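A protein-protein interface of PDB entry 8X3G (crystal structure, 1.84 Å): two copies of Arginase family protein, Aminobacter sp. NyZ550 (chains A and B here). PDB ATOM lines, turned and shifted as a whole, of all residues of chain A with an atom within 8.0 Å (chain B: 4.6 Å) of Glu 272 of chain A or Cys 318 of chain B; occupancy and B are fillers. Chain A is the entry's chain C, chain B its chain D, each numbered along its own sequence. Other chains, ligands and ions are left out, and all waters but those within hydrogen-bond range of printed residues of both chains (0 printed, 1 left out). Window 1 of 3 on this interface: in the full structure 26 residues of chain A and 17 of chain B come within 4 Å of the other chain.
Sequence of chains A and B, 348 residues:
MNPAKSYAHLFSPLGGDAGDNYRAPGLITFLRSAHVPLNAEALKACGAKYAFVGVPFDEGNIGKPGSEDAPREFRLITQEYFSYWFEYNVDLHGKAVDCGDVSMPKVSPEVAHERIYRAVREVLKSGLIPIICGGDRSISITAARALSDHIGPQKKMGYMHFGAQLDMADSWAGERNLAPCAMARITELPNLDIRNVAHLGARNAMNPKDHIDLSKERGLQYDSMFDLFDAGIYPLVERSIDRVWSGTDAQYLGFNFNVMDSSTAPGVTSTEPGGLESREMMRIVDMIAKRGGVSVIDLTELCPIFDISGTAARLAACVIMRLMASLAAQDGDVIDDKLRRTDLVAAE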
ATOM      1  N   LYS A  64     -30.726 -16.985 -24.526  1.00  0.00           N
ATOM      2  CA  LYS A  64     -30.160 -17.773 -23.403  1.00  0.00           C
ATOM      3  C   LYS A  64     -31.280 -18.560 -22.730  1.00  0.00           C
ATOM      4  O   LYS A  64     -32.361 -18.008 -22.527  1.00  0.00           O
ATOM      5  CB  LYS A  64     -29.455 -16.866 -22.395  1.00  0.00           C
ATOM      6  CG  LYS A  64     -28.174 -16.224 -22.912  1.00  0.00           C
ATOM      7  CD  LYS A  64     -27.525 -15.273 -21.928  1.00  0.00           C
ATOM      8  CE  LYS A  64     -27.545 -13.832 -22.387  1.00  0.00           C
ATOM      9  NZ  LYS A  64     -27.672 -12.895 -21.247  1.00  0.00           N
ATOM     10  N   ALA A 164     -36.850  -4.300 -22.783  1.00  0.00           N
ATOM     11  CA  ALA A 164     -35.772  -3.726 -23.592  1.00  0.00           C
ATOM     12  C   ALA A 164     -35.918  -4.046 -25.072  1.00  0.00           C
ATOM     13  O   ALA A 164     -35.311  -3.340 -25.900  1.00  0.00           O
ATOM     14  CB  ALA A 164     -34.417  -4.273 -23.140  1.00  0.00           C
ATOM     15  N   GLY A 201     -39.397   1.031 -22.870  1.00  0.00           N
ATOM     16  CA  GLY A 201     -38.050   0.599 -22.455  1.00  0.00           C
ATOM     17  C   GLY A 201     -37.101   0.195 -23.592  1.00  0.00           C
ATOM     18  O   GLY A 201     -35.957  -0.201 -23.291  1.00  0.00           O
ATOM     19  N   ALA A 202     -37.491   0.287 -24.878  1.00  0.00           N
ATOM     20  CA  ALA A 202     -36.663  -0.280 -25.951  1.00  0.00           C
ATOM     21  C   ALA A 202     -35.233   0.266 -25.892  1.00  0.00           C
ATOM     22  O   ALA A 202     -35.024   1.463 -25.668  1.00  0.00           O
ATOM     23  CB  ALA A 202     -37.255   0.056 -27.329  1.00  0.00           C
ATOM     24  N   ARG A 203     -34.240  -0.618 -26.094  1.00  0.00           N
ATOM     25  CA  ARG A 203     -32.833  -0.241 -25.947  1.00  0.00           C
ATOM     26  C   ARG A 203     -32.056  -0.348 -27.255  1.00  0.00           C
ATOM     27  O   ARG A 203     -32.291  -1.251 -28.066  1.00  0.00           O
ATOM     28  CB  ARG A 203     -32.128  -1.167 -24.943  1.00  0.00           C
ATOM     29  CG  ARG A 203     -32.725  -1.079 -23.482  1.00  0.00           C
ATOM     30  CD  ARG A 203     -32.527   0.317 -22.903  1.00  0.00           C
ATOM     31  NE  ARG A 203     -31.161   0.790 -23.025  1.00  0.00           N
ATOM     32  CZ  ARG A 203     -30.171   0.405 -22.215  1.00  0.00           C
ATOM     33  NH1 ARG A 203     -30.392  -0.457 -21.232  1.00  0.00           N
ATOM     34  NH2 ARG A 203     -28.924   0.826 -22.461  1.00  0.00           N
ATOM     35  N   ASN A 204     -31.058   0.519 -27.418  1.00  0.00           N
ATOM     36  CA  ASN A 204     -30.104   0.327 -28.493  1.00  0.00           C
ATOM     37  C   ASN A 204     -29.446  -1.047 -28.345  1.00  0.00           C
ATOM     38  O   ASN A 204     -29.289  -1.565 -27.236  1.00  0.00           O
ATOM     39  CB  ASN A 204     -28.967   1.347 -28.386  1.00  0.00           C
ATOM     40  CG  ASN A 204     -29.367   2.754 -28.753  1.00  0.00           C
ATOM     41  OD1 ASN A 204     -29.747   2.995 -29.896  1.00  0.00           O
ATOM     42  ND2 ASN A 204     -29.231   3.719 -27.780  1.00  0.00           N
ATOM     43  N   ALA A 205     -28.955  -1.556 -29.469  1.00  0.00           N
ATOM     44  CA  ALA A 205     -28.255  -2.824 -29.666  1.00  0.00           C
ATOM     45  C   ALA A 205     -29.027  -4.065 -29.207  1.00  0.00           C
ATOM     46  O   ALA A 205     -28.490  -5.176 -29.265  1.00  0.00           O
ATOM     47  CB  ALA A 205     -26.882  -2.776 -28.989  1.00  0.00           C
ATOM     48  N   MET A 206     -30.288  -3.932 -28.828  1.00  0.00           N
ATOM     49  CA  MET A 206     -31.172  -5.060 -28.577  1.00  0.00           C
ATOM     50  C   MET A 206     -32.314  -5.139 -29.597  1.00  0.00           C
ATOM     51  O   MET A 206     -33.185  -5.993 -29.455  1.00  0.00           O
ATOM     52  CB  MET A 206     -31.684  -4.921 -27.136  1.00  0.00           C
ATOM     53  CG  MET A 206     -30.512  -4.608 -26.158  1.00  0.00           C
ATOM     54  SD  MET A 206     -30.910  -4.941 -24.370  1.00  0.00           S
ATOM     55  CE  MET A 206     -31.765  -6.576 -24.311  1.00  0.00           C
ATOM     56  N   ASN A 207     -32.305  -4.297 -30.636  1.00  0.00           N
ATOM     57  CA  ASN A 207     -33.465  -4.090 -31.512  1.00  0.00           C
ATOM     58  C   ASN A 207     -33.009  -3.903 -32.957  1.00  0.00           C
ATOM     59  O   ASN A 207     -32.472  -2.836 -33.319  1.00  0.00           O
ATOM     60  CB  ASN A 207     -34.278  -2.882 -31.059  1.00  0.00           C
ATOM     61  CG  ASN A 207     -35.119  -3.210 -29.829  1.00  0.00           C
ATOM     62  OD1 ASN A 207     -36.102  -3.950 -29.918  1.00  0.00           O
ATOM     63  ND2 ASN A 207     -34.667  -2.764 -28.669  1.00  0.00           N
ATOM     64  N   MET A 225     -36.150   3.765 -24.107  1.00  0.00           N
ATOM     65  CA  MET A 225     -35.517   4.205 -22.871  1.00  0.00           C
ATOM     66  C   MET A 225     -35.070   5.665 -22.951  1.00  0.00           C
ATOM     67  O   MET A 225     -35.277   6.442 -22.007  1.00  0.00           O
ATOM     68  CB  MET A 225     -34.348   3.271 -22.556  1.00  0.00           C
ATOM     69  CG  MET A 225     -34.008   3.157 -21.086  1.00  0.00           C
ATOM     70  SD  MET A 225     -35.286   2.634 -19.936  1.00  0.00           S
ATOM     71  CE  MET A 225     -35.536   4.155 -19.037  1.00  0.00           C
ATOM     72  N   ASN A 258     -35.939  -7.264 -17.949  1.00  0.00           N
ATOM     73  CA  ASN A 258     -34.785  -6.598 -18.552  1.00  0.00           C
ATOM     74  C   ASN A 258     -35.068  -5.131 -18.851  1.00  0.00           C
ATOM     75  O   ASN A 258     -34.171  -4.414 -19.306  1.00  0.00           O
ATOM     76  CB  ASN A 258     -34.260  -7.383 -19.780  1.00  0.00           C
ATOM     77  CG  ASN A 258     -35.141  -7.227 -21.038  1.00  0.00           C
ATOM     78  OD1 ASN A 258     -36.180  -6.568 -21.028  1.00  0.00           O
ATOM     79  ND2 ASN A 258     -34.731  -7.899 -22.116  1.00  0.00           N
ATOM     80  N   VAL A 259     -36.278  -4.653 -18.585  1.00  0.00           N
ATOM     81  CA  VAL A 259     -36.496  -3.206 -18.593  1.00  0.00           C
ATOM     82  C   VAL A 259     -35.674  -2.526 -17.478  1.00  0.00           C
ATOM     83  O   VAL A 259     -35.438  -1.298 -17.531  1.00  0.00           O
ATOM     84  CB  VAL A 259     -38.000  -2.882 -18.464  1.00  0.00           C
ATOM     85  CG1 VAL A 259     -38.496  -3.082 -17.008  1.00  0.00           C
ATOM     86  CG2 VAL A 259     -38.307  -1.454 -18.910  1.00  0.00           C
ATOM     87  N   MET A 260     -35.361  -3.269 -16.397  1.00  0.00           N
ATOM     88  CA  MET A 260     -34.566  -2.762 -15.269  1.00  0.00           C
ATOM     89  C   MET A 260     -33.084  -2.753 -15.562  1.00  0.00           C
ATOM     90  O   MET A 260     -32.557  -3.624 -16.255  1.00  0.00           O
ATOM     91  CB  MET A 260     -34.804  -3.599 -14.002  1.00  0.00           C
ATOM     92  CG  MET A 260     -36.290  -3.954 -13.907  1.00  0.00           C
ATOM     93  SD  MET A 260     -37.311  -2.459 -13.460  1.00  0.00           S
ATOM     94  CE  MET A 260     -36.476  -1.645 -12.019  1.00  0.00           C
ATOM     95  N   ASP A 261     -32.404  -1.797 -14.945  1.00  0.00           N
ATOM     96  CA  ASP A 261     -30.957  -1.744 -15.021  1.00  0.00           C
ATOM     97  C   ASP A 261     -30.415  -3.103 -14.574  1.00  0.00           C
ATOM     98  O   ASP A 261     -30.968  -3.722 -13.666  1.00  0.00           O
ATOM     99  CB  ASP A 261     -30.466  -0.576 -14.133  1.00  0.00           C
ATOM    100  CG  ASP A 261     -29.009  -0.209 -14.382  1.00  0.00           C
ATOM    101  OD1 ASP A 261     -28.512  -0.401 -15.498  1.00  0.00           O
ATOM    102  OD2 ASP A 261     -28.424   0.445 -13.518  1.00  0.00           O
ATOM    103  N   SER A 262     -29.394  -3.593 -15.278  1.00  0.00           N
ATOM    104  CA  SER A 262     -28.940  -4.975 -15.066  1.00  0.00           C
ATOM    105  C   SER A 262     -28.622  -5.268 -13.598  1.00  0.00           C
ATOM    106  O   SER A 262     -28.876  -6.380 -13.121  1.00  0.00           O
ATOM    107  CB  SER A 262     -27.734  -5.258 -15.949  1.00  0.00           C
ATOM    108  OG  SER A 262     -28.070  -4.851 -17.260  1.00  0.00           O
ATOM    109  N   SER A 263     -28.087  -4.285 -12.876  1.00  0.00           N
ATOM    110  CA  SER A 263     -27.728  -4.432 -11.437  1.00  0.00           C
ATOM    111  C   SER A 263     -28.945  -4.822 -10.586  1.00  0.00           C
ATOM    112  O   SER A 263     -28.746  -5.488  -9.567  1.00  0.00           O
ATOM    113  CB  SER A 263     -27.144  -3.132 -10.952  1.00  0.00           C
ATOM    114  OG  SER A 263     -28.088  -2.080 -11.025  1.00  0.00           O
ATOM    115  N   ALA A 265     -31.719  -6.478 -11.883  1.00  0.00           N
ATOM    116  CA  ALA A 265     -32.381  -7.676 -12.451  1.00  0.00           C
ATOM    117  C   ALA A 265     -31.391  -8.468 -13.319  1.00  0.00           C
ATOM    118  O   ALA A 265     -31.542  -8.487 -14.530  1.00  0.00           O
ATOM    119  CB  ALA A 265     -33.608  -7.249 -13.204  1.00  0.00           C
ATOM    120  N   VAL A 268     -32.189 -12.499 -15.866  1.00  0.00           N
ATOM    121  CA  VAL A 268     -33.148 -12.375 -16.964  1.00  0.00           C
ATOM    122  C   VAL A 268     -32.434 -12.895 -18.214  1.00  0.00           C
ATOM    123  O   VAL A 268     -31.202 -13.005 -18.243  1.00  0.00           O
ATOM    124  CB  VAL A 268     -33.632 -10.926 -17.197  1.00  0.00           C
ATOM    125  CG1 VAL A 268     -34.387 -10.320 -15.944  1.00  0.00           C
ATOM    126  CG2 VAL A 268     -32.419 -10.008 -17.486  1.00  0.00           C
ATOM    127  N   SER A 270     -31.976 -11.716 -21.286  1.00  0.00           N
ATOM    128  CA  SER A 270     -31.027 -10.847 -22.001  1.00  0.00           C
ATOM    129  C   SER A 270     -31.048  -9.459 -21.346  1.00  0.00           C
ATOM    130  O   SER A 270     -32.117  -8.930 -21.075  1.00  0.00           O
ATOM    131  CB  SER A 270     -31.381 -10.783 -23.503  1.00  0.00           C
ATOM    132  OG  SER A 270     -32.584 -10.070 -23.620  1.00  0.00           O
ATOM    133  N   THR A 271     -29.895  -8.863 -21.097  1.00  0.00           N
ATOM    134  CA  THR A 271     -29.942  -7.571 -20.417  1.00  0.00           C
ATOM    135  C   THR A 271     -28.792  -6.707 -20.893  1.00  0.00           C
ATOM    136  O   THR A 271     -27.802  -7.191 -21.458  1.00  0.00           O
ATOM    137  CB  THR A 271     -29.878  -7.683 -18.898  1.00  0.00           C
ATOM    138  OG1 THR A 271     -30.135  -6.363 -18.354  1.00  0.00           O
ATOM    139  CG2 THR A 271     -28.477  -8.204 -18.532  1.00  0.00           C
ATOM    140  N   GLU A 272     -28.985  -5.398 -20.734  1.00  0.00           N
ATOM    141  CA  GLU A 272     -27.954  -4.414 -21.083  1.00  0.00           C
ATOM    142  C   GLU A 272     -28.091  -3.327 -20.024  1.00  0.00           C
ATOM    143  O   GLU A 272     -29.175  -2.800 -19.842  1.00  0.00           O
ATOM    144  CB  GLU A 272     -28.196  -3.876 -22.512  1.00  0.00           C
ATOM    145  CG  GLU A 272     -27.428  -2.698 -22.891  1.00  0.00           C
ATOM    146  CD  GLU A 272     -27.492  -2.452 -24.397  1.00  0.00           C
ATOM    147  OE1 GLU A 272     -28.580  -2.023 -24.858  1.00  0.00           O
ATOM    148  OE2 GLU A 272     -26.429  -2.557 -25.079  1.00  0.00           O
ATOM    149  N   PRO A 273     -27.021  -2.929 -19.359  1.00  0.00           N
ATOM    150  CA  PRO A 273     -27.169  -1.898 -18.325  1.00  0.00           C
ATOM    151  C   PRO A 273     -27.705  -0.598 -18.932  1.00  0.00           C
ATOM    152  O   PRO A 273     -27.516  -0.322 -20.107  1.00  0.00           O
ATOM    153  CB  PRO A 273     -25.733  -1.771 -17.748  1.00  0.00           C
ATOM    154  CG  PRO A 273     -24.927  -2.540 -18.548  1.00  0.00           C
ATOM    155  CD  PRO A 273     -25.722  -3.604 -19.240  1.00  0.00           C
ATOM    156  N   GLY A 274     -28.423   0.179 -18.125  1.00  0.00           N
ATOM    157  CA  GLY A 274     -28.932   1.504 -18.509  1.00  0.00           C
ATOM    158  C   GLY A 274     -30.454   1.570 -18.546  1.00  0.00           C
ATOM    159  O   GLY A 274     -31.028   2.516 -19.098  1.00  0.00           O
ATOM    160  N   GLY A 275     -31.119   0.665 -17.816  1.00  0.00           N
ATOM    161  CA  GLY A 275     -32.576   0.600 -17.738  1.00  0.00           C
ATOM    162  C   GLY A 275     -33.097   1.296 -16.475  1.00  0.00           C
ATOM    163  O   GLY A 275     -32.413   2.108 -15.838  1.00  0.00           O
ATOM    164  N   LEU A 276     -34.312   0.977 -16.112  1.00  0.00           N
ATOM    165  CA  LEU A 276     -34.985   1.624 -14.973  1.00  0.00           C
ATOM    166  C   LEU A 276     -34.395   1.195 -13.616  1.00  0.00           C
ATOM    167  O   LEU A 276     -33.915   0.070 -13.450  1.00  0.00           O
ATOM    168  CB  LEU A 276     -36.483   1.264 -14.967  1.00  0.00           C
ATOM    169  CG  LEU A 276     -37.380   1.810 -16.083  1.00  0.00           C
ATOM    170  CD1 LEU A 276     -38.760   1.222 -15.926  1.00  0.00           C
ATOM    171  CD2 LEU A 276     -37.494   3.322 -15.946  1.00  0.00           C
ATOM    172  N   TYR B  81     -24.899  -8.661 -28.701  1.00  0.00           N
ATOM    173  CA  TYR B  81     -25.566  -7.407 -29.007  1.00  0.00           C
ATOM    174  C   TYR B  81     -25.676  -7.246 -30.499  1.00  0.00           C
ATOM    175  O   TYR B  81     -24.829  -7.720 -31.252  1.00  0.00           O
ATOM    176  CB  TYR B  81     -24.823  -6.216 -28.387  1.00  0.00           C
ATOM    177  CG  TYR B  81     -24.966  -6.297 -26.875  1.00  0.00           C
ATOM    178  CD1 TYR B  81     -26.231  -6.117 -26.269  1.00  0.00           C
ATOM    179  CD2 TYR B  81     -23.881  -6.615 -26.070  1.00  0.00           C
ATOM    180  CE1 TYR B  81     -26.400  -6.226 -24.880  1.00  0.00           C
ATOM    181  CE2 TYR B  81     -24.028  -6.730 -24.666  1.00  0.00           C
ATOM    182  CZ  TYR B  81     -25.318  -6.537 -24.072  1.00  0.00           C
ATOM    183  OH  TYR B  81     -25.496  -6.676 -22.676  1.00  0.00           O
ATOM    184  N   TRP B  85     -27.694   0.647 -33.750  1.00  0.00           N
ATOM    185  CA  TRP B  85     -27.967   1.557 -32.634  1.00  0.00           C
ATOM    186  C   TRP B  85     -29.085   2.458 -33.142  1.00  0.00           C
ATOM    187  O   TRP B  85     -28.836   3.494 -33.744  1.00  0.00           O
ATOM    188  CB  TRP B  85     -26.656   2.338 -32.223  1.00  0.00           C
ATOM    189  CG  TRP B  85     -25.794   1.443 -31.412  1.00  0.00           C
ATOM    190  CD1 TRP B  85     -25.189   0.310 -31.831  1.00  0.00           C
ATOM    191  CD2 TRP B  85     -25.571   1.523 -29.990  1.00  0.00           C
ATOM    192  NE1 TRP B  85     -24.577  -0.319 -30.770  1.00  0.00           N
ATOM    193  CE2 TRP B  85     -24.816   0.400 -29.626  1.00  0.00           C
ATOM    194  CE3 TRP B  85     -25.972   2.432 -28.996  1.00  0.00           C
ATOM    195  CZ2 TRP B  85     -24.400   0.158 -28.301  1.00  0.00           C
ATOM    196  CZ3 TRP B  85     -25.556   2.201 -27.657  1.00  0.00           C
ATOM    197  CH2 TRP B  85     -24.762   1.066 -27.344  1.00  0.00           C
ATOM    198  N   MET B 282     -23.108   6.754 -19.530  1.00  0.00           N
ATOM    199  CA  MET B 282     -23.613   6.814 -20.924  1.00  0.00           C
ATOM    200  C   MET B 282     -23.744   8.284 -21.360  1.00  0.00           C
ATOM    201  O   MET B 282     -23.388   8.594 -22.492  1.00  0.00           O
ATOM    202  CB  MET B 282     -24.951   6.088 -21.050  1.00  0.00           C
ATOM    203  CG  MET B 282     -24.880   4.620 -20.730  1.00  0.00           C
ATOM    204  SD  MET B 282     -23.552   3.786 -21.613  1.00  0.00           S
ATOM    205  CE  MET B 282     -23.837   2.097 -21.092  1.00  0.00           C
ATOM    206  N   ARG B 314     -20.763  -6.442 -19.326  1.00  0.00           N
ATOM    207  CA  ARG B 314     -21.791  -5.839 -20.177  1.00  0.00           C
ATOM    208  C   ARG B 314     -21.754  -4.329 -20.089  1.00  0.00           C
ATOM    209  O   ARG B 314     -22.024  -3.618 -21.085  1.00  0.00           O
ATOM    210  CB  ARG B 314     -23.204  -6.318 -19.731  1.00  0.00           C
ATOM    211  CG  ARG B 314     -23.556  -7.734 -20.050  1.00  0.00           C
ATOM    212  CD  ARG B 314     -24.789  -8.190 -19.165  1.00  0.00           C
ATOM    213  NE  ARG B 314     -24.784  -9.635 -18.995  1.00  0.00           N
ATOM    214  CZ  ARG B 314     -24.949 -10.416 -20.032  1.00  0.00           C
ATOM    215  NH1 ARG B 314     -25.130  -9.902 -21.233  1.00  0.00           N
ATOM    216  NH2 ARG B 314     -24.897 -11.735 -19.872  1.00  0.00           N
ATOM    217  N   LEU B 315     -21.552  -3.804 -18.886  1.00  0.00           N
ATOM    218  CA  LEU B 315     -21.460  -2.353 -18.760  1.00  0.00           C
ATOM    219  C   LEU B 315     -20.313  -1.838 -19.606  1.00  0.00           C
ATOM    220  O   LEU B 315     -20.477  -0.896 -20.393  1.00  0.00           O
ATOM    221  CB  LEU B 315     -21.277  -1.959 -17.295  1.00  0.00           C
ATOM    222  CG  LEU B 315     -21.202  -0.473 -16.890  1.00  0.00           C
ATOM    223  CD1 LEU B 315     -19.815   0.122 -17.187  1.00  0.00           C
ATOM    224  CD2 LEU B 315     -22.310   0.334 -17.504  1.00  0.00           C
ATOM    225  N   ALA B 316     -19.143  -2.483 -19.479  1.00  0.00           N
ATOM    226  CA  ALA B 316     -17.993  -2.094 -20.284  1.00  0.00           C
ATOM    227  C   ALA B 316     -18.342  -2.126 -21.773  1.00  0.00           C
ATOM    228  O   ALA B 316     -18.022  -1.194 -22.538  1.00  0.00           O
ATOM    229  CB  ALA B 316     -16.826  -3.045 -19.954  1.00  0.00           C
ATOM    230  N   ALA B 317     -18.970  -3.211 -22.219  1.00  0.00           N
ATOM    231  CA  ALA B 317     -19.269  -3.348 -23.653  1.00  0.00           C
ATOM    232  C   ALA B 317     -20.214  -2.238 -24.098  1.00  0.00           C
ATOM    233  O   ALA B 317     -20.072  -1.673 -25.194  1.00  0.00           O
ATOM    234  CB  ALA B 317     -19.902  -4.718 -23.953  1.00  0.00           C
ATOM    235  N   CYS B 318     -21.224  -1.946 -23.277  1.00  0.00           N
ATOM    236  CA  CYS B 318     -22.192  -0.918 -23.670  1.00  0.00           C
ATOM    237  C   CYS B 318     -21.543   0.438 -23.711  1.00  0.00           C
ATOM    238  O   CYS B 318     -21.821   1.217 -24.629  1.00  0.00           O
ATOM    239  CB  CYS B 318     -23.396  -0.929 -22.722  1.00  0.00           C
ATOM    240  SG  CYS B 318     -24.230  -2.469 -23.044  1.00  0.00           S
ATOM    241  N   VAL B 319     -20.627   0.705 -22.785  1.00  0.00           N
ATOM    242  CA  VAL B 319     -19.916   1.994 -22.803  1.00  0.00           C
ATOM    243  C   VAL B 319     -19.070   2.112 -24.077  1.00  0.00           C
ATOM    244  O   VAL B 319     -19.112   3.138 -24.779  1.00  0.00           O
ATOM    245  CB  VAL B 319     -19.059   2.178 -21.524  1.00  0.00           C
ATOM    246  CG1 VAL B 319     -18.067   3.341 -21.677  1.00  0.00           C
ATOM    247  CG2 VAL B 319     -19.941   2.364 -20.305  1.00  0.00           C
ATOM    248  N   ILE B 320     -18.304   1.069 -24.402  1.00  0.00           N
ATOM    249  CA  ILE B 320     -17.437   1.136 -25.596  1.00  0.00           C
ATOM    250  C   ILE B 320     -18.277   1.258 -26.875  1.00  0.00           C
ATOM    251  O   ILE B 320     -17.986   2.060 -27.769  1.00  0.00           O
ATOM    252  CB  ILE B 320     -16.511  -0.094 -25.664  1.00  0.00           C
ATOM    253  CG1 ILE B 320     -15.581  -0.132 -24.438  1.00  0.00           C
ATOM    254  CG2 ILE B 320     -15.747  -0.082 -27.015  1.00  0.00           C
ATOM    255  CD1 ILE B 320     -14.662   1.100 -24.295  1.00  0.00           C
ATOM    256  N   MET B 321     -19.319   0.427 -27.005  1.00  0.00           N
ATOM    257  CA  MET B 321     -20.093   0.422 -28.242  1.00  0.00           C
ATOM    258  C   MET B 321     -20.879   1.713 -28.367  1.00  0.00           C
ATOM    259  O   MET B 321     -21.028   2.262 -29.473  1.00  0.00           O
ATOM    260  CB  MET B 321     -20.988  -0.819 -28.233  1.00  0.00           C
ATOM    261  CG  MET B 321     -20.167  -2.089 -28.484  1.00  0.00           C
ATOM    262  SD  MET B 321     -21.189  -3.615 -28.540  1.00  0.00           S
ATOM    263  CE  MET B 321     -22.427  -3.289 -27.370  1.00  0.00           C
ATOM    264  N   ARG B 322     -21.369   2.229 -27.249  1.00  0.00           N
ATOM    265  CA  ARG B 322     -22.099   3.490 -27.309  1.00  0.00           C
ATOM    266  C   ARG B 322     -21.169   4.636 -27.705  1.00  0.00           C
ATOM    267  O   ARG B 322     -21.578   5.554 -28.426  1.00  0.00           O
ATOM    268  CB  ARG B 322     -22.736   3.781 -25.948  1.00  0.00           C
ATOM    269  CG  ARG B 322     -23.411   5.163 -25.876  1.00  0.00           C
ATOM    270  CD  ARG B 322     -24.876   5.056 -25.499  1.00  0.00           C
ATOM    271  NE  ARG B 322     -25.445   6.378 -25.243  1.00  0.00           N
ATOM    272  CZ  ARG B 322     -26.373   6.674 -24.341  1.00  0.00           C
ATOM    273  NH1 ARG B 322     -26.952   5.729 -23.612  1.00  0.00           N
ATOM    274  NH2 ARG B 322     -26.780   7.945 -24.223  1.00  0.00           N
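OH of Tyr 81 of chain B sits at hydrogen-bond distance from O of Thr 271 of chain A (2.7 Å). The side-chain amino group (NZ) of Lys 64 of chain A lies close to the guanidinium group (NH2) of Arg 314 of chain B (3.3 Å). The side-chain sulfur (SG) of Cys 318 of chain B sits at hydrogen-bond distance from the side-chain carboxylate (OE2) of Glu 272 of chain A (3.0 Å).
The backbone carbonyl oxygen of Asn 204 of chain A sits close to the side-chain carboxylate of Glu 272 of chain A (2.5 Å). The guanidinium group (NH2) of Arg 203 of chain A lies within salt-bridge range of the side-chain carboxylate (OE1) of Glu 272 of chain A, 3.7 Å away. The side-chain hydroxyl (OG1) of Thr 271 of chain A sits at hydrogen-bond distance from the side-chain hydroxyl (OG) of Ser 262 of chain A. The backbone carbonyl oxygen (O) of Arg 314 of chain B sits at hydrogen-bond distance from the side-chain sulfur (SG) of Cys 318 of chain B, at 3.2 Å. The side-chain hydroxyl (OG) of Ser 262 of chain A sits close to the backbone carbonyl oxygen (O) of Glu 272 of chain A, 3.5 Å away. O of Pro 273 of chain A lies within hydrogen-bond range of NH2 of Arg 203 of chain A, at 3.0 Å.
Among the printed residues, merely in contact across the chains: Asn 204 of chain A with Trp 85 of chain B (3.2 Å), Ala 205 of chain A with Tyr 81 of chain B (3.7 Å), Ala 205 of chain A with Trp 85 of chain B (3.8 Å), Thr 271 of chain A with Arg 314 of chain B (3.7 Å), Glu 272 of chain A with Tyr 81 of chain B (3.7 Å), Pro 273 of chain A with Arg 314 of chain B (3.7 Å) and Pro 273 of chain A with Leu 315 of chain B (3.5 Å).
Ala 265 of chain A touches none of the printed residues of chain B. Of chain B, only Tyr 81 (3.7 Å) and Cys 318 (3.0 Å) come within 4 Å of Glu 272 of chain A. Of the printed residues of chain A, Tyr 81 of chain B touches Ala 205, Thr 271 and Glu 272. Of the printed residues of chain A, Arg 314 of chain B touches Lys 64, Thr 271 and Pro 273. No residue of chain A comes within 4 Å of Ala 317 of chain B. Of the printed residues of chain A, Cys 318 of chain B touches Glu 272 (3.0 Å). The nearest printed residue of chain B that does not touch Glu 272 of chain A is Trp 85 of chain B (4.6 Å). The nearest residue of chain A that does not touch Cys 318 of chain B is Pro 273 of chain A (4.2 Å). The nearest printed residue of chain B that does not touch Lys 64 of chain A is Tyr 81 of chain B (6.7 Å).
Of the 12 printed residues of chain B, 5 touch a printed residue of chain A. Of the 25 printed residues of chain A, 6 touch a printed residue of chain B.
No position is printed for both chains.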
